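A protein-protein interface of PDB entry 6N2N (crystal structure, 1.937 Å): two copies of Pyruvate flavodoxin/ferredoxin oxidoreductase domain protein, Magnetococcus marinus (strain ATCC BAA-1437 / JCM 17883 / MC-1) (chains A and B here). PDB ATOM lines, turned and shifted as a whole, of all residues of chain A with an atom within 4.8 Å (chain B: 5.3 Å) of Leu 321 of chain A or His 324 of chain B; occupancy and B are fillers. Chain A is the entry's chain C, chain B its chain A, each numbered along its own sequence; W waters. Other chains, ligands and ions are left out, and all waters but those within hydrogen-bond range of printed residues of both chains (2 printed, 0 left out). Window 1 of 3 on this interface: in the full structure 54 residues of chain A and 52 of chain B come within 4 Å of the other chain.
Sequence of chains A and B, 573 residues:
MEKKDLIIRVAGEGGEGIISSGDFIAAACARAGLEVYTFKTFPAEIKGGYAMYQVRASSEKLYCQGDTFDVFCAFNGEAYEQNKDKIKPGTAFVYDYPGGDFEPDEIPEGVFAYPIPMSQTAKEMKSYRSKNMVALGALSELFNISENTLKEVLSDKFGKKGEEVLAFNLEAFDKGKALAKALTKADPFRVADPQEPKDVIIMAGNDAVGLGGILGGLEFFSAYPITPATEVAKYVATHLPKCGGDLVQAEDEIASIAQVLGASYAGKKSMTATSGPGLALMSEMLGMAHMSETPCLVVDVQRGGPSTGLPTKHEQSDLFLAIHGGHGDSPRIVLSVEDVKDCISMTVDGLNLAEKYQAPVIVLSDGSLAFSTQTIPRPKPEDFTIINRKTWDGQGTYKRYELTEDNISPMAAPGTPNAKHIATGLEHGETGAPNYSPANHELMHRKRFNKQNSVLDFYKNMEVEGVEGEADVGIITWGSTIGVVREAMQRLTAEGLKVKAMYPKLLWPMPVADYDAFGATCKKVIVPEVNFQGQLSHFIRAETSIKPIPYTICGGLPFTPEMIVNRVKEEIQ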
ATOM      1  N   GLY A 276      29.252  21.924 -27.213  1.00  0.00           N
ATOM      2  CA  GLY A 276      27.921  21.349 -27.134  1.00  0.00           C
ATOM      3  C   GLY A 276      27.457  20.572 -28.352  1.00  0.00           C
ATOM      4  O   GLY A 276      27.037  19.417 -28.238  1.00  0.00           O
ATOM      5  N   LEU A 279      29.460  17.349 -28.537  1.00  0.00           N
ATOM      6  CA  LEU A 279      29.101  16.384 -27.506  1.00  0.00           C
ATOM      7  C   LEU A 279      27.791  15.680 -27.846  1.00  0.00           C
ATOM      8  O   LEU A 279      27.630  14.488 -27.565  1.00  0.00           O
ATOM      9  CB  LEU A 279      29.008  17.068 -26.140  1.00  0.00           C
ATOM     10  CG  LEU A 279      28.671  16.106 -24.992  1.00  0.00           C
ATOM     11  CD1 LEU A 279      29.725  14.997 -24.886  1.00  0.00           C
ATOM     12  CD2 LEU A 279      28.499  16.819 -23.659  1.00  0.00           C
ATOM     13  N   ALA A 280      26.844  16.400 -28.456  1.00  0.00           N
ATOM     14  CA  ALA A 280      25.582  15.775 -28.846  1.00  0.00           C
ATOM     15  C   ALA A 280      25.802  14.709 -29.912  1.00  0.00           C
ATOM     16  O   ALA A 280      25.186  13.636 -29.866  1.00  0.00           O
ATOM     17  CB  ALA A 280      24.597  16.835 -29.344  1.00  0.00           C
ATOM     18  N   SER A 283      27.067  11.242 -28.500  1.00  0.00           N
ATOM     19  CA  SER A 283      26.254  10.527 -27.516  1.00  0.00           C
ATOM     20  C   SER A 283      26.260   9.019 -27.750  1.00  0.00           C
ATOM     21  O   SER A 283      26.419   8.243 -26.800  1.00  0.00           O
ATOM     22  CB  SER A 283      24.822  11.068 -27.528  1.00  0.00           C
ATOM     23  OG  SER A 283      24.788  12.413 -27.046  1.00  0.00           O
ATOM     24  N   ASP A 318      25.339  22.563 -20.601  1.00  0.00           N
ATOM     25  CA  ASP A 318      25.497  21.207 -21.114  1.00  0.00           C
ATOM     26  C   ASP A 318      25.492  20.148 -20.011  1.00  0.00           C
ATOM     27  O   ASP A 318      25.894  19.007 -20.258  1.00  0.00           O
ATOM     28  CB  ASP A 318      26.788  21.086 -21.934  1.00  0.00           C
ATOM     29  CG  ASP A 318      26.720  21.826 -23.270  1.00  0.00           C
ATOM     30  OD1 ASP A 318      25.631  22.308 -23.639  1.00  0.00           O
ATOM     31  OD2 ASP A 318      27.764  21.914 -23.960  1.00  0.00           O
ATOM     32  N   LEU A 319      25.049  20.495 -18.801  1.00  0.00           N
ATOM     33  CA  LEU A 319      25.038  19.515 -17.717  1.00  0.00           C
ATOM     34  C   LEU A 319      23.996  18.429 -17.965  1.00  0.00           C
ATOM     35  O   LEU A 319      24.239  17.250 -17.680  1.00  0.00           O
ATOM     36  CB  LEU A 319      24.778  20.209 -16.381  1.00  0.00           C
ATOM     37  CG  LEU A 319      24.873  19.314 -15.137  1.00  0.00           C
ATOM     38  CD1 LEU A 319      26.276  18.693 -15.009  1.00  0.00           C
ATOM     39  CD2 LEU A 319      24.497  20.094 -13.884  1.00  0.00           C
ATOM     40  N   PHE A 320      22.827  18.811 -18.484  1.00  0.00           N
ATOM     41  CA  PHE A 320      21.805  17.829 -18.836  1.00  0.00           C
ATOM     42  C   PHE A 320      22.335  16.819 -19.853  1.00  0.00           C
ATOM     43  O   PHE A 320      22.200  15.603 -19.665  1.00  0.00           O
ATOM     44  CB  PHE A 320      20.564  18.537 -19.383  1.00  0.00           C
ATOM     45  CG  PHE A 320      19.652  19.121 -18.318  1.00  0.00           C
ATOM     46  CD1 PHE A 320      19.839  18.829 -16.973  1.00  0.00           C
ATOM     47  CD2 PHE A 320      18.584  19.943 -18.680  1.00  0.00           C
ATOM     48  CE1 PHE A 320      18.989  19.354 -16.004  1.00  0.00           C
ATOM     49  CE2 PHE A 320      17.728  20.471 -17.718  1.00  0.00           C
ATOM     50  CZ  PHE A 320      17.924  20.173 -16.379  1.00  0.00           C
ATOM     51  N   LEU A 321      22.954  17.310 -20.931  1.00  0.00           N
ATOM     52  CA  LEU A 321      23.484  16.426 -21.968  1.00  0.00           C
ATOM     53  C   LEU A 321      24.627  15.564 -21.443  1.00  0.00           C
ATOM     54  O   LEU A 321      24.716  14.375 -21.767  1.00  0.00           O
ATOM     55  CB  LEU A 321      23.957  17.248 -23.171  1.00  0.00           C
ATOM     56  CG  LEU A 321      24.782  16.501 -24.227  1.00  0.00           C
ATOM     57  CD1 LEU A 321      23.985  15.365 -24.852  1.00  0.00           C
ATOM     58  CD2 LEU A 321      25.287  17.453 -25.307  1.00  0.00           C
ATOM     59  N   ALA A 322      25.520  16.148 -20.645  1.00  0.00           N
ATOM     60  CA  ALA A 322      26.667  15.392 -20.155  1.00  0.00           C
ATOM     61  C   ALA A 322      26.224  14.221 -19.286  1.00  0.00           C
ATOM     62  O   ALA A 322      26.800  13.129 -19.360  1.00  0.00           O
ATOM     63  CB  ALA A 322      27.602  16.322 -19.378  1.00  0.00           C
ATOM     64  N   ILE A 323      25.189  14.415 -18.479  1.00  0.00           N
ATOM     65  CA  ILE A 323      24.765  13.371 -17.555  1.00  0.00           C
ATOM     66  C   ILE A 323      23.766  12.416 -18.205  1.00  0.00           C
ATOM     67  O   ILE A 323      23.868  11.200 -18.032  1.00  0.00           O
ATOM     68  CB  ILE A 323      24.196  14.006 -16.268  1.00  0.00           C
ATOM     69  CG1 ILE A 323      25.297  14.775 -15.527  1.00  0.00           C
ATOM     70  CG2 ILE A 323      23.578  12.931 -15.364  1.00  0.00           C
ATOM     71  CD1 ILE A 323      24.811  15.530 -14.293  1.00  0.00           C
ATOM     72  N   HIS A 324      22.813  12.931 -18.987  1.00  0.00           N
ATOM     73  CA  HIS A 324      21.696  12.134 -19.495  1.00  0.00           C
ATOM     74  C   HIS A 324      21.715  11.949 -21.006  1.00  0.00           C
ATOM     75  O   HIS A 324      20.700  11.538 -21.575  1.00  0.00           O
ATOM     76  CB  HIS A 324      20.363  12.771 -19.089  1.00  0.00           C
ATOM     77  CG  HIS A 324      19.984  12.518 -17.666  1.00  0.00           C
ATOM     78  ND1 HIS A 324      19.045  13.274 -16.999  1.00  0.00           N
ATOM     79  CD2 HIS A 324      20.421  11.591 -16.780  1.00  0.00           C
ATOM     80  CE1 HIS A 324      18.920  12.825 -15.762  1.00  0.00           C
ATOM     81  NE2 HIS A 324      19.744  11.804 -15.605  1.00  0.00           N
ATOM     82  N   GLY A 325      22.830  12.232 -21.670  1.00  0.00           N
ATOM     83  CA  GLY A 325      22.845  12.210 -23.116  1.00  0.00           C
ATOM     84  C   GLY A 325      22.856  10.857 -23.790  1.00  0.00           C
ATOM     85  O   GLY A 325      22.775  10.803 -25.019  1.00  0.00           O
ATOM     86  N   ARG A 332      27.738   8.582 -17.257  1.00  0.00           N
ATOM     87  CA  ARG A 332      29.063   9.153 -17.448  1.00  0.00           C
ATOM     88  C   ARG A 332      29.580   9.687 -16.120  1.00  0.00           C
ATOM     89  O   ARG A 332      28.806  10.004 -15.212  1.00  0.00           O
ATOM     90  CB  ARG A 332      29.051  10.303 -18.475  1.00  0.00           C
ATOM     91  CG  ARG A 332      28.645   9.902 -19.880  1.00  0.00           C
ATOM     92  CD  ARG A 332      27.133   9.939 -20.076  1.00  0.00           C
ATOM     93  NE  ARG A 332      26.801   9.681 -21.472  1.00  0.00           N
ATOM     94  CZ  ARG A 332      26.599  10.624 -22.384  1.00  0.00           C
ATOM     95  NH1 ARG A 332      26.668  11.911 -22.050  1.00  0.00           N
ATOM     96  NH2 ARG A 332      26.317  10.275 -23.635  1.00  0.00           N
ATOM     97  N   HIS A 538      18.216  21.220 -10.696  1.00  0.00           N
ATOM     98  CA  HIS A 538      17.409  20.056 -11.048  1.00  0.00           C
ATOM     99  C   HIS A 538      17.948  18.786 -10.393  1.00  0.00           C
ATOM    100  O   HIS A 538      17.184  17.994  -9.831  1.00  0.00           O
ATOM    101  CB  HIS A 538      17.348  19.896 -12.568  1.00  0.00           C
ATOM    102  CG  HIS A 538      16.818  18.568 -13.011  1.00  0.00           C
ATOM    103  ND1 HIS A 538      15.491  18.364 -13.323  1.00  0.00           N
ATOM    104  CD2 HIS A 538      17.433  17.375 -13.187  1.00  0.00           C
ATOM    105  CE1 HIS A 538      15.312  17.104 -13.676  1.00  0.00           C
ATOM    106  NE2 HIS A 538      16.474  16.481 -13.596  1.00  0.00           N
ATOM    107  N   LEU B 319      14.048   7.533 -21.509  1.00  0.00           N
ATOM    108  CA  LEU B 319      13.382   8.741 -21.026  1.00  0.00           C
ATOM    109  C   LEU B 319      14.387   9.854 -20.742  1.00  0.00           C
ATOM    110  O   LEU B 319      14.137  11.020 -21.068  1.00  0.00           O
ATOM    111  CB  LEU B 319      12.550   8.422 -19.781  1.00  0.00           C
ATOM    112  CG  LEU B 319      11.707   9.580 -19.232  1.00  0.00           C
ATOM    113  CD1 LEU B 319      10.746  10.097 -20.296  1.00  0.00           C
ATOM    114  CD2 LEU B 319      10.939   9.152 -17.990  1.00  0.00           C
ATOM    115  N   PHE B 320      15.534   9.512 -20.152  1.00  0.00           N
ATOM    116  CA  PHE B 320      16.580  10.504 -19.920  1.00  0.00           C
ATOM    117  C   PHE B 320      17.031  11.140 -21.232  1.00  0.00           C
ATOM    118  O   PHE B 320      17.154  12.365 -21.335  1.00  0.00           O
ATOM    119  CB  PHE B 320      17.768   9.852 -19.206  1.00  0.00           C
ATOM    120  CG  PHE B 320      17.569   9.641 -17.723  1.00  0.00           C
ATOM    121  CD1 PHE B 320      16.493  10.199 -17.057  1.00  0.00           C
ATOM    122  CD2 PHE B 320      18.477   8.875 -16.996  1.00  0.00           C
ATOM    123  CE1 PHE B 320      16.319   9.998 -15.687  1.00  0.00           C
ATOM    124  CE2 PHE B 320      18.315   8.680 -15.631  1.00  0.00           C
ATOM    125  CZ  PHE B 320      17.234   9.240 -14.976  1.00  0.00           C
ATOM    126  N   LEU B 321      17.293  10.312 -22.247  1.00  0.00           N
ATOM    127  CA  LEU B 321      17.746  10.819 -23.538  1.00  0.00           C
ATOM    128  C   LEU B 321      16.674  11.661 -24.227  1.00  0.00           C
ATOM    129  O   LEU B 321      16.986  12.700 -24.818  1.00  0.00           O
ATOM    130  CB  LEU B 321      18.174   9.652 -24.433  1.00  0.00           C
ATOM    131  CG  LEU B 321      18.433  10.016 -25.896  1.00  0.00           C
ATOM    132  CD1 LEU B 321      19.547  11.032 -25.987  1.00  0.00           C
ATOM    133  CD2 LEU B 321      18.778   8.790 -26.717  1.00  0.00           C
ATOM    134  N   ALA B 322      15.409  11.225 -24.184  1.00  0.00           N
ATOM    135  CA  ALA B 322      14.356  11.976 -24.867  1.00  0.00           C
ATOM    136  C   ALA B 322      14.190  13.369 -24.271  1.00  0.00           C
ATOM    137  O   ALA B 322      13.916  14.336 -24.994  1.00  0.00           O
ATOM    138  CB  ALA B 322      13.029  11.214 -24.809  1.00  0.00           C
ATOM    139  N   ILE B 323      14.340  13.492 -22.957  1.00  0.00           N
ATOM    140  CA  ILE B 323      14.105  14.773 -22.303  1.00  0.00           C
ATOM    141  C   ILE B 323      15.362  15.633 -22.267  1.00  0.00           C
ATOM    142  O   ILE B 323      15.294  16.838 -22.515  1.00  0.00           O
ATOM    143  CB  ILE B 323      13.533  14.543 -20.889  1.00  0.00           C
ATOM    144  CG1 ILE B 323      12.157  13.871 -20.989  1.00  0.00           C
ATOM    145  CG2 ILE B 323      13.459  15.872 -20.114  1.00  0.00           C
ATOM    146  CD1 ILE B 323      11.545  13.501 -19.651  1.00  0.00           C
ATOM    147  N   HIS B 324      16.524  15.040 -21.980  1.00  0.00           N
ATOM    148  CA  HIS B 324      17.747  15.797 -21.723  1.00  0.00           C
ATOM    149  C   HIS B 324      18.836  15.581 -22.776  1.00  0.00           C
ATOM    150  O   HIS B 324      19.993  15.955 -22.542  1.00  0.00           O
ATOM    151  CB  HIS B 324      18.294  15.446 -20.333  1.00  0.00           C
ATOM    152  CG  HIS B 324      17.557  16.108 -19.206  1.00  0.00           C
ATOM    153  ND1 HIS B 324      17.652  15.677 -17.900  1.00  0.00           N
ATOM    154  CD2 HIS B 324      16.728  17.180 -19.189  1.00  0.00           C
ATOM    155  CE1 HIS B 324      16.909  16.449 -17.128  1.00  0.00           C
ATOM    156  NE2 HIS B 324      16.340  17.371 -17.884  1.00  0.00           N
ATOM    157  N   GLY B 325      18.504  15.006 -23.929  1.00  0.00           N
ATOM    158  CA  GLY B 325      19.504  14.654 -24.923  1.00  0.00           C
ATOM    159  C   GLY B 325      20.092  15.805 -25.727  1.00  0.00           C
ATOM    160  O   GLY B 325      21.013  15.572 -26.514  1.00  0.00           O
ATOM    161  N   GLY B 326      19.612  17.029 -25.559  1.00  0.00           N
ATOM    162  CA  GLY B 326      20.090  18.151 -26.338  1.00  0.00           C
ATOM    163  C   GLY B 326      21.101  18.968 -25.556  1.00  0.00           C
ATOM    164  O   GLY B 326      21.008  19.088 -24.339  1.00  0.00           O
ATOM    165  N   HIS B 327      22.092  19.502 -26.267  1.00  0.00           N
ATOM    166  CA  HIS B 327      23.031  20.420 -25.634  1.00  0.00           C
ATOM    167  C   HIS B 327      22.363  21.770 -25.418  1.00  0.00           C
ATOM    168  O   HIS B 327      21.434  22.150 -26.139  1.00  0.00           O
ATOM    169  CB  HIS B 327      24.304  20.577 -26.473  1.00  0.00           C
ATOM    170  CG  HIS B 327      24.114  21.330 -27.752  1.00  0.00           C
ATOM    171  ND1 HIS B 327      23.625  20.745 -28.901  1.00  0.00           N
ATOM    172  CD2 HIS B 327      24.388  22.618 -28.074  1.00  0.00           C
ATOM    173  CE1 HIS B 327      23.589  21.643 -29.869  1.00  0.00           C
ATOM    174  NE2 HIS B 327      24.044  22.789 -29.393  1.00  0.00           N
ATOM    175  N   ARG B 332      12.296  19.099 -25.444  1.00  0.00           N
ATOM    176  CA  ARG B 332      11.439  18.366 -26.364  1.00  0.00           C
ATOM    177  C   ARG B 332      10.082  18.124 -25.709  1.00  0.00           C
ATOM    178  O   ARG B 332       9.946  18.149 -24.483  1.00  0.00           O
ATOM    179  CB  ARG B 332      12.054  17.011 -26.767  1.00  0.00           C
ATOM    180  CG  ARG B 332      13.383  17.076 -27.539  1.00  0.00           C
ATOM    181  CD  ARG B 332      14.600  17.155 -26.617  1.00  0.00           C
ATOM    182  NE  ARG B 332      15.840  17.040 -27.380  1.00  0.00           N
ATOM    183  CZ  ARG B 332      16.488  15.896 -27.571  1.00  0.00           C
ATOM    184  NH1 ARG B 332      16.026  14.768 -27.036  1.00  0.00           N
ATOM    185  NH2 ARG B 332      17.598  15.874 -28.294  1.00  0.00           N
ATOM    186  N   HIS B 538      12.926   9.694 -11.090  1.00  0.00           N
ATOM    187  CA  HIS B 538      13.873  10.801 -11.060  1.00  0.00           C
ATOM    188  C   HIS B 538      13.174  12.126 -11.335  1.00  0.00           C
ATOM    189  O   HIS B 538      13.366  13.105 -10.605  1.00  0.00           O
ATOM    190  CB  HIS B 538      14.987  10.553 -12.082  1.00  0.00           C
ATOM    191  CG  HIS B 538      15.844  11.751 -12.354  1.00  0.00           C
ATOM    192  ND1 HIS B 538      17.043  11.973 -11.713  1.00  0.00           N
ATOM    193  CD2 HIS B 538      15.672  12.795 -13.199  1.00  0.00           C
ATOM    194  CE1 HIS B 538      17.572  13.102 -12.150  1.00  0.00           C
ATOM    195  NE2 HIS B 538      16.758  13.622 -13.049  1.00  0.00           N
ATOM    196  N   PHE B 539      12.353  12.178 -12.386  1.00  0.00           N
ATOM    197  CA  PHE B 539      11.671  13.426 -12.717  1.00  0.00           C
ATOM    198  C   PHE B 539      10.555  13.740 -11.729  1.00  0.00           C
ATOM    199  O   PHE B 539      10.282  14.917 -11.461  1.00  0.00           O
ATOM    200  CB  PHE B 539      11.144  13.369 -14.147  1.00  0.00           C
ATOM    201  CG  PHE B 539      12.226  13.494 -15.177  1.00  0.00           C
ATOM    202  CD1 PHE B 539      12.803  14.728 -15.447  1.00  0.00           C
ATOM    203  CD2 PHE B 539      12.691  12.377 -15.857  1.00  0.00           C
ATOM    204  CE1 PHE B 539      13.813  14.847 -16.388  1.00  0.00           C
ATOM    205  CE2 PHE B 539      13.706  12.486 -16.799  1.00  0.00           C
ATOM    206  CZ  PHE B 539      14.269  13.722 -17.061  1.00  0.00           C
HETATM  207  O   HOH W   1      22.238  13.151 -26.599  1.00  0.00           O
HETATM  208  O   HOH W   2      22.486  20.073 -21.835  1.00  0.00           O
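Water W1 lies within hydrogen-bond range of OG of Ser 283 of chain A (2.7 Å), O of Gly 325 of chain B (2.7 Å) and O of Gly 325 of chain A (2.9 Å).
Water W2 bridges N of Leu 321 of chain A and O of Gly 326 of chain B.
O of Leu 321 of chain B sits at hydrogen-bond distance from NH1 of Arg 332 of chain B, at 3.2 Å.
OG of Ser 283 of chain A lies close to O of Gly 325 of chain A, at 3.3 Å.
O of Leu 321 of chain A sits at hydrogen-bond distance from NH1 of Arg 332 of chain A, 3.2 Å away.
Gly 276 of chain A touches His 327 of chain B.
Phe 320 of chain A touches His 324 of chain B.
CA of Leu 321 of chain A touches O of His 324 of chain B, at 3.6 Å.
O of Gly 325 of chain B touches CD1 of Leu 321 of chain A, 3.4 Å away.
Gly 326 of chain B touches Leu 321 of chain A (O to CB, 3.7 Å).
CB of His 327 of chain B touches CD2 of Leu 321 of chain A, at 3.5 Å.
His 324 of chain A touches Phe 320 of chain B (CD2 to CD2, 3.3 Å).
O of Gly 325 of chain A touches CD1 of Leu 321 of chain B, at 3.4 Å.
CE1 of His 324 of chain B touches NE2 of His 538 of chain A, 3.6 Å away.
CE1 of Phe 539 of chain B touches CE1 of His 538 of chain A, at 3.8 Å.
ND1 of His 324 of chain B sits at hydrogen-bond distance from ND1 of His 324 of chain A, at 2.9 Å.
A ring nitrogen (NE2) of His 538 of chain B sits at hydrogen-bond distance from a ring nitrogen (NE2) of His 538 of chain A.
Leu 321 of chain A touches His 324 of chain B, and with the chains exchanged His 324 of chain A touches Leu 321 of chain B.
Leu 321 of chain A touches Gly 325 of chain B, and with the chains exchanged Gly 325 of chain A touches Leu 321 of chain B.
His 324 of chain B touches its own counterpart, His 324 of chain A.
His 538 of chain B touches its own counterpart, His 538 of chain A.
Positions printed for both chains: 319, 320, 321, 322, 323, 324, 325, 332 and 538.
Of the printed residues of chain B, Asp 318 of chain A touches His 327 (3.6 Å).
Printed residues of chain B within 4 Å of Phe 320 of chain A: His 324 (3.4 Å).
Of the printed residues of chain B, Gly 325 of chain A touches Leu 321.
Printed residues of chain A within 4 Å of Leu 321 of chain B: His 324 and Gly 325.
His 324 of chain B touches just these residues of chain A: Phe 320 (3.4 Å), Leu 321 (3.6 Å), His 324 (2.9 Å) and His 538 (3.6 Å).
Of the printed residues of chain A, His 538 of chain B touches His 324 (3.6 Å) and His 538 (2.9 Å).
The nearest printed residue of chain B that does not touch Leu 321 of chain A is Leu 321 of chain B (6.3 Å).
The nearest residue of chain A that does not touch His 324 of chain B is Gly 325 of chain A (4.7 Å).
The nearest printed residue of chain B that does not touch Gly 325 of chain A is Gly 325 of chain B (4.5 Å).
Printed residues of chain B that touch a printed residue of chain A: Phe 320, Leu 321, His 324, Gly 325, Gly 326, His 327, His 538 and Phe 539.
Hydrophobic or aromatic side chains of chain B within 4 Å of the printed part of chain A: Phe 320, Leu 321, His 324, His 327, His 538 and Phe 539.
Of the 14 printed residues of chain A, 7 touch a printed residue of chain B.
Printed residues of chain A that touch a printed residue of chain B: Gly 276, Asp 318, Phe 320, Leu 321, His 324, Gly 325 and His 538.
Hydrophobic or aromatic side chains of chain A within 4 Å of the printed part of chain B: Phe 320, Leu 321, His 324 and His 538.
Among the printed residues, no Asp or Glu carboxylate lies within 4 Å of a Lys or Arg side-chain nitrogen of the other chain.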
